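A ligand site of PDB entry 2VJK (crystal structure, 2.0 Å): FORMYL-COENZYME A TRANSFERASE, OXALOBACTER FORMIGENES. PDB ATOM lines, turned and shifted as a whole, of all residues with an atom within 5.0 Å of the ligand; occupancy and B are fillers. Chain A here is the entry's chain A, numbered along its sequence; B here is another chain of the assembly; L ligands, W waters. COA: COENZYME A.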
ATOM      1  N   HIS A  15      29.573   1.155 -25.141  1.00  0.00           N
ATOM      2  CA  HIS A  15      28.153   0.940 -25.307  1.00  0.00           C
ATOM      3  C   HIS A  15      27.463   2.258 -25.682  1.00  0.00           C
ATOM      4  O   HIS A  15      28.069   3.330 -25.625  1.00  0.00           O
ATOM      5  CB  HIS A  15      27.550   0.356 -24.032  1.00  0.00           C
ATOM      6  CG  HIS A  15      27.610   1.278 -22.860  1.00  0.00           C
ATOM      7  ND1 HIS A  15      26.498   1.584 -22.107  1.00  0.00           N
ATOM      8  CD2 HIS A  15      28.635   1.988 -22.331  1.00  0.00           C
ATOM      9  CE1 HIS A  15      26.841   2.439 -21.147  1.00  0.00           C
ATOM     10  NE2 HIS A  15      28.129   2.693 -21.259  1.00  0.00           N
ATOM     11  N   VAL A  16      26.198   2.153 -26.065  1.00  0.00           N
ATOM     12  CA  VAL A  16      25.375   3.297 -26.513  1.00  0.00           C
ATOM     13  C   VAL A  16      26.015   4.071 -27.707  1.00  0.00           C
ATOM     14  O   VAL A  16      26.268   3.464 -28.750  1.00  0.00           O
ATOM     15  CB  VAL A  16      24.817   4.126 -25.302  1.00  0.00           C
ATOM     16  CG1 VAL A  16      25.920   4.765 -24.472  1.00  0.00           C
ATOM     17  CG2 VAL A  16      23.775   5.149 -25.762  1.00  0.00           C
ATOM     18  N   GLN A  17      26.305   5.372 -27.591  1.00  0.00           N
ATOM     19  CA  GLN A  17      26.654   6.169 -28.791  1.00  0.00           C
ATOM     20  C   GLN A  17      28.126   6.547 -28.971  1.00  0.00           C
ATOM     21  O   GLN A  17      28.737   6.211 -29.973  1.00  0.00           O
ATOM     22  CB  GLN A  17      25.825   7.451 -28.848  1.00  0.00           C
ATOM     23  CG  GLN A  17      24.327   7.246 -28.980  1.00  0.00           C
ATOM     24  CD  GLN A  17      23.546   8.242 -28.148  1.00  0.00           C
ATOM     25  OE1 GLN A  17      22.879   9.135 -28.693  1.00  0.00           O
ATOM     26  NE2 GLN A  17      23.611   8.102 -26.824  1.00  0.00           N
ATOM     27  N   ALA A  18      28.691   7.274 -27.995  1.00  0.00           N
ATOM     28  CA  ALA A  18      29.997   7.933 -28.158  1.00  0.00           C
ATOM     29  C   ALA A  18      31.157   6.965 -28.384  1.00  0.00           C
ATOM     30  O   ALA A  18      31.916   7.095 -29.343  1.00  0.00           O
ATOM     31  CB  ALA A  18      30.295   8.828 -26.957  1.00  0.00           C
ATOM     32  N   ILE A  36      33.057  -6.152 -26.169  1.00  0.00           N
ATOM     33  CA  ILE A  36      32.616  -6.854 -24.969  1.00  0.00           C
ATOM     34  C   ILE A  36      31.227  -6.374 -24.561  1.00  0.00           C
ATOM     35  O   ILE A  36      31.008  -5.177 -24.398  1.00  0.00           O
ATOM     36  CB  ILE A  36      33.553  -6.607 -23.772  1.00  0.00           C
ATOM     37  CG1 ILE A  36      34.965  -7.093 -24.079  1.00  0.00           C
ATOM     38  CG2 ILE A  36      33.011  -7.307 -22.531  1.00  0.00           C
ATOM     39  CD1 ILE A  36      35.949  -6.807 -22.990  1.00  0.00           C
ATOM     40  N   GLU A  37      30.316  -7.327 -24.362  1.00  0.00           N
ATOM     41  CA  GLU A  37      28.942  -6.991 -24.061  1.00  0.00           C
ATOM     42  C   GLU A  37      28.429  -7.755 -22.853  1.00  0.00           C
ATOM     43  O   GLU A  37      28.919  -8.824 -22.527  1.00  0.00           O
ATOM     44  CB  GLU A  37      28.043  -7.285 -25.265  1.00  0.00           C
ATOM     45  CG  GLU A  37      28.431  -6.512 -26.495  1.00  0.00           C
ATOM     46  CD  GLU A  37      27.382  -6.564 -27.554  1.00  0.00           C
ATOM     47  OE1 GLU A  37      26.267  -6.059 -27.310  1.00  0.00           O
ATOM     48  OE2 GLU A  37      27.667  -7.110 -28.640  1.00  0.00           O
ATOM     49  N   ARG A  38      27.429  -7.168 -22.202  1.00  0.00           N
ATOM     50  CA  ARG A  38      26.781  -7.786 -21.059  1.00  0.00           C
ATOM     51  C   ARG A  38      25.983  -9.000 -21.538  1.00  0.00           C
ATOM     52  O   ARG A  38      25.375  -8.959 -22.607  1.00  0.00           O
ATOM     53  CB  ARG A  38      25.859  -6.773 -20.380  1.00  0.00           C
ATOM     54  CG  ARG A  38      25.670  -6.989 -18.899  1.00  0.00           C
ATOM     55  CD  ARG A  38      24.522  -6.144 -18.384  1.00  0.00           C
ATOM     56  NE  ARG A  38      24.793  -4.710 -18.480  1.00  0.00           N
ATOM     57  CZ  ARG A  38      25.428  -3.983 -17.551  1.00  0.00           C
ATOM     58  NH1 ARG A  38      25.892  -4.556 -16.440  1.00  0.00           N
ATOM     59  NH2 ARG A  38      25.606  -2.687 -17.748  1.00  0.00           N
ATOM     60  N   LEU A  72      30.285 -11.305 -21.852  1.00  0.00           N
ATOM     61  CA  LEU A  72      31.191 -11.452 -20.727  1.00  0.00           C
ATOM     62  C   LEU A  72      30.638 -10.795 -19.469  1.00  0.00           C
ATOM     63  O   LEU A  72      30.238  -9.624 -19.490  1.00  0.00           O
ATOM     64  CB  LEU A  72      32.562 -10.846 -21.074  1.00  0.00           C
ATOM     65  CG  LEU A  72      33.744 -11.186 -20.159  1.00  0.00           C
ATOM     66  CD1 LEU A  72      33.990 -12.691 -20.100  1.00  0.00           C
ATOM     67  CD2 LEU A  72      34.992 -10.466 -20.618  1.00  0.00           C
ATOM     68  N   ASP A  73      30.597 -11.563 -18.381  1.00  0.00           N
ATOM     69  CA  ASP A  73      30.326 -11.018 -17.053  1.00  0.00           C
ATOM     70  C   ASP A  73      31.690 -10.685 -16.456  1.00  0.00           C
ATOM     71  O   ASP A  73      32.456 -11.591 -16.109  1.00  0.00           O
ATOM     72  CB  ASP A  73      29.569 -12.036 -16.179  1.00  0.00           C
ATOM     73  CG  ASP A  73      29.017 -11.416 -14.895  1.00  0.00           C
ATOM     74  OD1 ASP A  73      29.632 -10.470 -14.359  1.00  0.00           O
ATOM     75  OD2 ASP A  73      27.960 -11.880 -14.430  1.00  0.00           O
ATOM     76  N   MET A  74      31.989  -9.393 -16.379  1.00  0.00           N
ATOM     77  CA  MET A  74      33.290  -8.925 -15.904  1.00  0.00           C
ATOM     78  C   MET A  74      33.351  -8.791 -14.379  1.00  0.00           C
ATOM     79  O   MET A  74      34.419  -8.503 -13.821  1.00  0.00           O
ATOM     80  CB  MET A  74      33.640  -7.597 -16.575  1.00  0.00           C
ATOM     81  CG  MET A  74      33.716  -7.678 -18.098  1.00  0.00           C
ATOM     82  SD  MET A  74      33.661  -6.063 -18.911  1.00  0.00           S
ATOM     83  CE  MET A  74      35.112  -5.292 -18.195  1.00  0.00           C
ATOM     84  N   LYS A  75      32.215  -8.986 -13.712  1.00  0.00           N
ATOM     85  CA  LYS A  75      32.140  -9.077 -12.251  1.00  0.00           C
ATOM     86  C   LYS A  75      32.151 -10.540 -11.791  1.00  0.00           C
ATOM     87  O   LYS A  75      31.381 -10.937 -10.913  1.00  0.00           O
ATOM     88  CB  LYS A  75      30.905  -8.341 -11.727  1.00  0.00           C
ATOM     89  CG  LYS A  75      30.963  -6.819 -11.916  1.00  0.00           C
ATOM     90  CD  LYS A  75      29.647  -6.146 -11.553  1.00  0.00           C
ATOM     91  CE  LYS A  75      29.762  -4.632 -11.614  1.00  0.00           C
ATOM     92  NZ  LYS A  75      28.518  -3.940 -11.167  1.00  0.00           N
ATOM     93  N   ASN A  96      33.305   3.656 -22.356  1.00  0.00           N
ATOM     94  CA  ASN A  96      32.463   4.808 -21.993  1.00  0.00           C
ATOM     95  C   ASN A  96      31.418   4.399 -20.955  1.00  0.00           C
ATOM     96  O   ASN A  96      30.220   4.662 -21.107  1.00  0.00           O
ATOM     97  CB  ASN A  96      31.864   5.531 -23.233  1.00  0.00           C
ATOM     98  CG  ASN A  96      30.807   4.722 -23.980  1.00  0.00           C
ATOM     99  OD1 ASN A  96      30.964   3.518 -24.187  1.00  0.00           O
ATOM    100  ND2 ASN A  96      29.748   5.398 -24.425  1.00  0.00           N
ATOM    101  N   PHE A  97      31.903   3.737 -19.914  1.00  0.00           N
ATOM    102  CA  PHE A  97      31.126   3.493 -18.700  1.00  0.00           C
ATOM    103  C   PHE A  97      31.059   4.805 -17.916  1.00  0.00           C
ATOM    104  O   PHE A  97      31.759   5.769 -18.245  1.00  0.00           O
ATOM    105  CB  PHE A  97      31.784   2.449 -17.794  1.00  0.00           C
ATOM    106  CG  PHE A  97      31.833   1.051 -18.359  1.00  0.00           C
ATOM    107  CD1 PHE A  97      33.009   0.308 -18.304  1.00  0.00           C
ATOM    108  CD2 PHE A  97      30.701   0.458 -18.912  1.00  0.00           C
ATOM    109  CE1 PHE A  97      33.062  -0.985 -18.811  1.00  0.00           C
ATOM    110  CE2 PHE A  97      30.750  -0.842 -19.413  1.00  0.00           C
ATOM    111  CZ  PHE A  97      31.933  -1.562 -19.359  1.00  0.00           C
ATOM    112  N   GLY A  98      30.252   4.817 -16.865  1.00  0.00           N
ATOM    113  CA  GLY A  98      30.216   5.935 -15.929  1.00  0.00           C
ATOM    114  C   GLY A  98      31.547   6.112 -15.228  1.00  0.00           C
ATOM    115  O   GLY A  98      32.356   5.181 -15.175  1.00  0.00           O
ATOM    116  N   PRO A  99      31.811   7.327 -14.687  1.00  0.00           N
ATOM    117  CA  PRO A  99      33.078   7.602 -13.992  1.00  0.00           C
ATOM    118  C   PRO A  99      33.435   6.563 -12.927  1.00  0.00           C
ATOM    119  O   PRO A  99      32.571   6.171 -12.140  1.00  0.00           O
ATOM    120  CB  PRO A  99      32.823   8.965 -13.341  1.00  0.00           C
ATOM    121  CG  PRO A  99      31.849   9.628 -14.263  1.00  0.00           C
ATOM    122  CD  PRO A  99      30.935   8.505 -14.712  1.00  0.00           C
ATOM    123  N   ALA A 101      33.977   3.391 -13.120  1.00  0.00           N
ATOM    124  CA  ALA A 101      33.465   2.021 -13.329  1.00  0.00           C
ATOM    125  C   ALA A 101      34.555   0.988 -13.623  1.00  0.00           C
ATOM    126  O   ALA A 101      34.536  -0.111 -13.053  1.00  0.00           O
ATOM    127  CB  ALA A 101      32.416   2.010 -14.427  1.00  0.00           C
ATOM    128  N   ARG A 104      36.678   0.275 -10.456  1.00  0.00           N
ATOM    129  CA  ARG A 104      35.968  -0.583  -9.510  1.00  0.00           C
ATOM    130  C   ARG A 104      35.993  -2.059  -9.905  1.00  0.00           C
ATOM    131  O   ARG A 104      35.898  -2.941  -9.053  1.00  0.00           O
ATOM    132  CB  ARG A 104      34.522  -0.095  -9.319  1.00  0.00           C
ATOM    133  CG  ARG A 104      34.419   1.231  -8.565  1.00  0.00           C
ATOM    134  CD  ARG A 104      33.012   1.535  -8.081  1.00  0.00           C
ATOM    135  NE  ARG A 104      32.116   1.997  -9.142  1.00  0.00           N
ATOM    136  CZ  ARG A 104      32.136   3.221  -9.684  1.00  0.00           C
ATOM    137  NH1 ARG A 104      32.998   4.135  -9.261  1.00  0.00           N
ATOM    138  NH2 ARG A 104      31.276   3.528 -10.649  1.00  0.00           N
ATOM    139  N   MET A 105      36.127  -2.324 -11.210  1.00  0.00           N
ATOM    140  CA  MET A 105      36.344  -3.684 -11.712  1.00  0.00           C
ATOM    141  C   MET A 105      37.753  -4.200 -11.418  1.00  0.00           C
ATOM    142  O   MET A 105      38.012  -5.389 -11.572  1.00  0.00           O
ATOM    143  CB  MET A 105      36.113  -3.748 -13.227  1.00  0.00           C
ATOM    144  CG  MET A 105      34.668  -3.657 -13.652  1.00  0.00           C
ATOM    145  SD  MET A 105      34.539  -3.747 -15.450  1.00  0.00           S
ATOM    146  CE  MET A 105      32.769  -3.592 -15.699  1.00  0.00           C
ATOM    147  N   VAL A 124      35.596   7.955 -22.848  1.00  0.00           N
ATOM    148  CA  VAL A 124      34.672   9.080 -22.960  1.00  0.00           C
ATOM    149  C   VAL A 124      33.931   9.196 -21.640  1.00  0.00           C
ATOM    150  O   VAL A 124      33.378   8.216 -21.152  1.00  0.00           O
ATOM    151  CB  VAL A 124      33.630   8.893 -24.085  1.00  0.00           C
ATOM    152  CG1 VAL A 124      32.636  10.078 -24.098  1.00  0.00           C
ATOM    153  CG2 VAL A 124      34.324   8.754 -25.440  1.00  0.00           C
ATOM    154  N   LYS A 125      33.956  10.401 -21.064  1.00  0.00           N
ATOM    155  CA  LYS A 125      33.202  10.735 -19.867  1.00  0.00           C
ATOM    156  C   LYS A 125      32.400  12.012 -20.103  1.00  0.00           C
ATOM    157  O   LYS A 125      32.617  12.705 -21.078  1.00  0.00           O
ATOM    158  CB  LYS A 125      34.145  10.915 -18.674  1.00  0.00           C
ATOM    159  CG  LYS A 125      34.952   9.664 -18.314  1.00  0.00           C
ATOM    160  CD  LYS A 125      34.094   8.630 -17.581  1.00  0.00           C
ATOM    161  CE  LYS A 125      34.721   7.231 -17.586  1.00  0.00           C
ATOM    162  NZ  LYS A 125      34.374   6.488 -18.823  1.00  0.00           N
ATOM    163  N   GLY A 126      31.462  12.318 -19.201  1.00  0.00           N
ATOM    164  CA  GLY A 126      30.667  13.544 -19.296  1.00  0.00           C
ATOM    165  C   GLY A 126      31.516  14.788 -19.075  1.00  0.00           C
ATOM    166  O   GLY A 126      31.469  15.742 -19.874  1.00  0.00           O
ATOM    167  N   LEU A 136      29.690  12.859 -12.655  1.00  0.00           N
ATOM    168  CA  LEU A 136      28.334  12.815 -13.202  1.00  0.00           C
ATOM    169  C   LEU A 136      28.180  11.937 -14.453  1.00  0.00           C
ATOM    170  O   LEU A 136      29.060  11.897 -15.316  1.00  0.00           O
ATOM    171  CB  LEU A 136      27.836  14.237 -13.503  1.00  0.00           C
ATOM    172  CG  LEU A 136      27.581  15.111 -12.282  1.00  0.00           C
ATOM    173  CD1 LEU A 136      27.107  16.471 -12.726  1.00  0.00           C
ATOM    174  CD2 LEU A 136      26.558  14.475 -11.338  1.00  0.00           C
ATOM    175  N   LYS A 137      27.053  11.241 -14.520  1.00  0.00           N
ATOM    176  CA  LYS A 137      26.632  10.516 -15.728  1.00  0.00           C
ATOM    177  C   LYS A 137      25.895  11.473 -16.663  1.00  0.00           C
ATOM    178  O   LYS A 137      24.904  12.094 -16.281  1.00  0.00           O
ATOM    179  CB  LYS A 137      25.723   9.330 -15.343  1.00  0.00           C
ATOM    180  CG  LYS A 137      26.484   8.184 -14.666  1.00  0.00           C
ATOM    181  CD  LYS A 137      25.557   7.063 -14.219  1.00  0.00           C
ATOM    182  CE  LYS A 137      26.352   5.906 -13.634  1.00  0.00           C
ATOM    183  NZ  LYS A 137      25.483   4.814 -13.086  1.00  0.00           N
ATOM    184  N   VAL A 138      26.390  11.591 -17.896  1.00  0.00           N
ATOM    185  CA  VAL A 138      25.869  12.583 -18.836  1.00  0.00           C
ATOM    186  C   VAL A 138      25.349  11.892 -20.104  1.00  0.00           C
ATOM    187  O   VAL A 138      25.946  10.915 -20.572  1.00  0.00           O
ATOM    188  CB  VAL A 138      26.966  13.630 -19.192  1.00  0.00           C
ATOM    189  CG1 VAL A 138      26.485  14.602 -20.264  1.00  0.00           C
ATOM    190  CG2 VAL A 138      27.394  14.377 -17.935  1.00  0.00           C
ATOM    191  N   TYR A 139      24.226  12.371 -20.609  1.00  0.00           N
ATOM    192  CA  TYR A 139      23.648  11.914 -21.877  1.00  0.00           C
ATOM    193  C   TYR A 139      23.728  13.033 -22.920  1.00  0.00           C
ATOM    194  O   TYR A 139      24.060  14.175 -22.585  1.00  0.00           O
ATOM    195  CB  TYR A 139      22.205  11.463 -21.652  1.00  0.00           C
ATOM    196  CG  TYR A 139      22.095  10.285 -20.705  1.00  0.00           C
ATOM    197  CD1 TYR A 139      22.181   8.970 -21.175  1.00  0.00           C
ATOM    198  CD2 TYR A 139      21.919  10.486 -19.336  1.00  0.00           C
ATOM    199  CE1 TYR A 139      22.090   7.894 -20.304  1.00  0.00           C
ATOM    200  CE2 TYR A 139      21.833   9.412 -18.457  1.00  0.00           C
ATOM    201  CZ  TYR A 139      21.921   8.122 -18.950  1.00  0.00           C
ATOM    202  OH  TYR A 139      21.831   7.071 -18.063  1.00  0.00           O
ATOM    203  N   GLU A 140      23.411  12.696 -24.177  1.00  0.00           N
ATOM    204  CA  GLU A 140      23.558  13.606 -25.325  1.00  0.00           C
ATOM    205  C   GLU A 140      23.191  15.074 -25.052  1.00  0.00           C
ATOM    206  O   GLU A 140      24.048  15.949 -25.088  1.00  0.00           O
ATOM    207  CB  GLU A 140      22.751  13.083 -26.529  1.00  0.00           C
ATOM    208  CG  GLU A 140      22.710  14.000 -27.757  1.00  0.00           C
ATOM    209  CD  GLU A 140      24.074  14.291 -28.346  1.00  0.00           C
ATOM    210  OE1 GLU A 140      24.418  15.480 -28.549  1.00  0.00           O
ATOM    211  OE2 GLU A 140      24.836  13.324 -28.625  1.00  0.00           O
ATOM    212  N   ASP A 169      27.595  13.087 -28.218  1.00  0.00           N
ATOM    213  CA  ASP A 169      28.006  11.689 -28.282  1.00  0.00           C
ATOM    214  C   ASP A 169      28.942  11.350 -29.421  1.00  0.00           C
ATOM    215  O   ASP A 169      30.122  11.145 -29.180  1.00  0.00           O
ATOM    216  CB  ASP A 169      26.770  10.808 -28.309  1.00  0.00           C
ATOM    217  CG  ASP A 169      26.268  10.611 -26.893  1.00  0.00           C
ATOM    218  OD1 ASP A 169      25.281  11.209 -26.517  1.00  0.00           O
ATOM    219  N   MET A 200      32.686  14.960 -22.723  1.00  0.00           N
ATOM    220  CA  MET A 200      31.622  15.364 -23.640  1.00  0.00           C
ATOM    221  C   MET A 200      31.445  16.868 -23.606  1.00  0.00           C
ATOM    222  O   MET A 200      31.254  17.487 -24.661  1.00  0.00           O
ATOM    223  CB  MET A 200      30.314  14.659 -23.285  1.00  0.00           C
ATOM    224  CG  MET A 200      30.338  13.143 -23.552  1.00  0.00           C
ATOM    225  SD  MET A 200      28.903  12.304 -22.863  1.00  0.00           S
ATOM    226  CE  MET A 200      27.631  12.843 -24.007  1.00  0.00           C
ATOM    227  N   ASN B 287      16.161   2.945 -16.007  1.00  0.00           N
ATOM    228  CA  ASN B 287      16.595   2.492 -14.672  1.00  0.00           C
ATOM    229  C   ASN B 287      16.394   3.532 -13.561  1.00  0.00           C
ATOM    230  O   ASN B 287      16.283   3.167 -12.389  1.00  0.00           O
ATOM    231  CB  ASN B 287      18.054   2.012 -14.700  1.00  0.00           C
ATOM    232  CG  ASN B 287      19.030   3.092 -15.189  1.00  0.00           C
ATOM    233  OD1 ASN B 287      18.649   4.005 -15.929  1.00  0.00           O
ATOM    234  ND2 ASN B 287      20.285   2.983 -14.770  1.00  0.00           N
ATOM    235  N   MET B 288      16.350   4.813 -13.931  1.00  0.00           N
ATOM    236  CA  MET B 288      16.200   5.910 -12.976  1.00  0.00           C
ATOM    237  C   MET B 288      14.740   6.348 -12.769  1.00  0.00           C
ATOM    238  O   MET B 288      14.492   7.364 -12.119  1.00  0.00           O
ATOM    239  CB  MET B 288      17.022   7.130 -13.429  1.00  0.00           C
ATOM    240  CG  MET B 288      18.523   6.863 -13.575  1.00  0.00           C
ATOM    241  SD  MET B 288      19.367   6.600 -12.003  1.00  0.00           S
ATOM    242  CE  MET B 288      21.042   6.268 -12.540  1.00  0.00           C
HETATM  243  N1A COA L   1      29.850  -7.067 -16.866  1.00  0.00           N
HETATM  244  C2A COA L   1      29.847  -6.640 -15.595  1.00  0.00           C
HETATM  245  N3A COA L   1      29.569  -5.355 -15.288  1.00  0.00           N
HETATM  246  C4A COA L   1      29.277  -4.463 -16.279  1.00  0.00           C
HETATM  247  C5A COA L   1      29.269  -4.888 -17.593  1.00  0.00           C
HETATM  248  C6A COA L   1      29.566  -6.217 -17.884  1.00  0.00           C
HETATM  249  N6A COA L   1      29.560  -6.657 -19.143  1.00  0.00           N
HETATM  250  N7A COA L   1      28.956  -3.823 -18.359  1.00  0.00           N
HETATM  251  C8A COA L   1      28.774  -2.764 -17.530  1.00  0.00           C
HETATM  252  N9A COA L   1      28.976  -3.156 -16.266  1.00  0.00           N
HETATM  253  C1B COA L   1      28.864  -2.328 -15.034  1.00  0.00           C
HETATM  254  C2B COA L   1      29.753  -1.091 -15.036  1.00  0.00           C
HETATM  255  O2B COA L   1      31.107  -1.393 -14.710  1.00  0.00           O
HETATM  256  C3B COA L   1      29.093  -0.269 -13.956  1.00  0.00           C
HETATM  257  O3B COA L   1      29.656  -0.649 -12.708  1.00  0.00           O
HETATM  258  P3B COA L   1      29.451   0.156 -11.332  1.00  0.00           P
HETATM  259  O7A COA L   1      29.101   1.577 -11.704  1.00  0.00           O
HETATM  260  O8A COA L   1      28.398  -0.595 -10.551  1.00  0.00           O
HETATM  261  O9A COA L   1      30.753  -0.047 -10.595  1.00  0.00           O
HETATM  262  C4B COA L   1      27.618  -0.646 -14.026  1.00  0.00           C
HETATM  263  O4B COA L   1      27.542  -1.809 -14.860  1.00  0.00           O
HETATM  264  C5B COA L   1      26.728   0.482 -14.550  1.00  0.00           C
HETATM  265  O5B COA L   1      27.082   0.813 -15.894  1.00  0.00           O
HETATM  266  P1A COA L   1      27.341   2.346 -16.344  1.00  0.00           P
HETATM  267  O1A COA L   1      27.392   2.412 -17.854  1.00  0.00           O
HETATM  268  O2A COA L   1      28.636   2.844 -15.750  1.00  0.00           O
HETATM  269  O3A COA L   1      26.132   3.191 -15.702  1.00  0.00           O
HETATM  270  P2A COA L   1      24.715   3.516 -16.408  1.00  0.00           P
HETATM  271  O4A COA L   1      23.755   3.833 -15.282  1.00  0.00           O
HETATM  272  O5A COA L   1      24.358   2.435 -17.401  1.00  0.00           O
HETATM  273  O6A COA L   1      25.002   4.912 -17.176  1.00  0.00           O
HETATM  274  CBP COA L   1      25.894   6.210 -19.019  1.00  0.00           C
HETATM  275  CCP COA L   1      24.966   5.064 -18.586  1.00  0.00           C
HETATM  276  CDP COA L   1      25.869   6.276 -20.542  1.00  0.00           C
HETATM  277  CEP COA L   1      25.324   7.506 -18.449  1.00  0.00           C
HETATM  278  CAP COA L   1      27.315   5.947 -18.501  1.00  0.00           C
HETATM  279  OAP COA L   1      27.803   4.715 -19.028  1.00  0.00           O
HETATM  280  C9P COA L   1      28.268   7.077 -18.844  1.00  0.00           C
HETATM  281  O9P COA L   1      28.314   8.180 -18.106  1.00  0.00           O
HETATM  282  N8P COA L   1      29.060   6.923 -19.919  1.00  0.00           N
HETATM  283  C7P COA L   1      30.022   7.938 -20.338  1.00  0.00           C
HETATM  284  C6P COA L   1      29.346   9.068 -21.103  1.00  0.00           C
HETATM  285  C5P COA L   1      28.568   8.544 -22.301  1.00  0.00           C
HETATM  286  O5P COA L   1      29.095   7.722 -23.068  1.00  0.00           O
HETATM  287  N4P COA L   1      27.341   9.050 -22.435  1.00  0.00           N
HETATM  288  C3P COA L   1      26.304   8.471 -23.281  1.00  0.00           C
HETATM  289  C2P COA L   1      25.924   9.410 -24.432  1.00  0.00           C
HETATM  290  S1P COA L   1      27.144   9.335 -25.705  1.00  0.00           S
HETATM  291  O   HOH W   1      26.495  -4.189 -13.003  1.00  0.00           O
HETATM  292  O   HOH W   2      29.232  -4.462 -21.020  1.00  0.00           O
HETATM  293  O   HOH W   3      28.663   3.714 -13.336  1.00  0.00           O
HETATM  294  O   HOH W   4      32.359  -1.559 -12.177  1.00  0.00           O
HETATM  295  O   HOH W   5      29.471  10.594 -17.769  1.00  0.00           O
HETATM  296  O   HOH W   6      27.890  -8.454 -13.852  1.00  0.00           O
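The side-chain amino group (NZ) of Lys 75 is in salt-bridge range of an oxygen (O8A) of the ligand. The backbone carbonyl oxygen (O) of Val 138 sits at hydrogen-bond distance from a nitrogen (N4P) of the ligand, 3.0 Å away. The side-chain amino group of Lys 137 lies within salt-bridge range of an oxygen (O4A) of the ligand, at 3.0 Å. NE2 of His 15 is in hydrogen-bond range of OAP of the ligand. S1P of the ligand is bonded to CG of Asp 169 (2.0 Å). The backbone NH (N) of Met 74 sits at hydrogen-bond distance from a nitrogen (N1A) of the ligand (3.2 Å). A nitrogen (N8P) of the ligand lies within hydrogen-bond range of the backbone carbonyl oxygen of Phe 97 (3.4 Å). O of Leu 72 is in hydrogen-bond range of N6A of the ligand (3.1 Å). N of Gly 98 sits at hydrogen-bond distance from O2A of the ligand (2.8 Å). The side-chain sulfur (SD) of Met 200 lies within hydrogen-bond range of a nitrogen (N4P) of the ligand (3.6 Å). N of Ala 18 lies close to S1P of the ligand (3.4 Å). An oxygen (O9A) of the ligand lies within salt-bridge range of the guanidinium group (NE) of Arg 104 (2.9 Å). An oxygen (O5P) of the ligand is in hydrogen-bond range of the side-chain amide nitrogen (ND2) of Asn 96, 2.8 Å away. The backbone carbonyl oxygen (O) of Asn 96 lies within hydrogen-bond range of a nitrogen (N8P) of the ligand (2.8 Å).
O of Phe 97 sits at hydrogen-bond distance from NZ of Lys 125, at 2.8 Å. NE2 of His 15 is in hydrogen-bond range of O of Asn 96 (2.9 Å). The backbone NH (N) of Met 200 is in hydrogen-bond range of the backbone carbonyl oxygen (O) of Lys 125 (2.8 Å). The backbone NH (N) of Met 200 lies within hydrogen-bond range of the backbone carbonyl oxygen (O) of Gly 126, 3.2 Å away. N of Leu 72 is in hydrogen-bond range of O of Glu 37, at 2.9 Å. The backbone NH of Lys 75 lies within hydrogen-bond range of the side-chain carboxylate of Asp 73 (3.0 Å). The guanidinium group of Arg 104 sits at hydrogen-bond distance from the backbone carbonyl oxygen of Pro 99, 3.3 Å away. The backbone NH of Asp 169 lies within hydrogen-bond range of the side-chain carboxylate of Glu 140.
N9A of the ligand sits close to NH1 of Arg 38 (3.4 Å). Residues that only touch the ligand: Val 16 (3.9 Å), Gln 17 (3.6 Å), Asp 73 (3.98 Å), Ala 101 (3.7 Å), Met 105 (2.9 Å), Val 124 (3.5 Å), Tyr 139 (3.5 Å) and Asn 287 of chain B (3.6 Å). Hydrophobic or aromatic side chains within 4 Å of the ligand: His 15, Val 16, Ala 18, Met 74, Phe 97, Ala 101, Met 105, Tyr 139 and Met 200. 22 residues have an atom within 4 Å of the ligand: His 15, Val 16, Gln 17, Ala 18, Arg 38, Leu 72, Asp 73, Met 74, Lys 75, Asn 96, Phe 97, Gly 98, Ala 101, Arg 104, Met 105, Val 124, Lys 137, Val 138, Tyr 139, Asp 169, Met 200 and Asn 287 of chain B.
Water W3 bridges O2A of the ligand (2.6 Å) and NZ of Lys 137 (3.4 Å). Water W5 lies within hydrogen-bond range of O9P of the ligand (2.7 Å), O of Leu 136 (2.8 Å), N of Gly 126 (3.0 Å) and N of Val 138 (3.2 Å). Water W4 bridges an oxygen (O9A) of the ligand (2.7 Å) and the backbone carbonyl oxygen (O) of Ala 101 (2.8 Å). Water W2 bridges N7A of the ligand and N of Arg 38. Water W1 lies within hydrogen-bond range of NZ of Lys 75 and O4B of the ligand.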
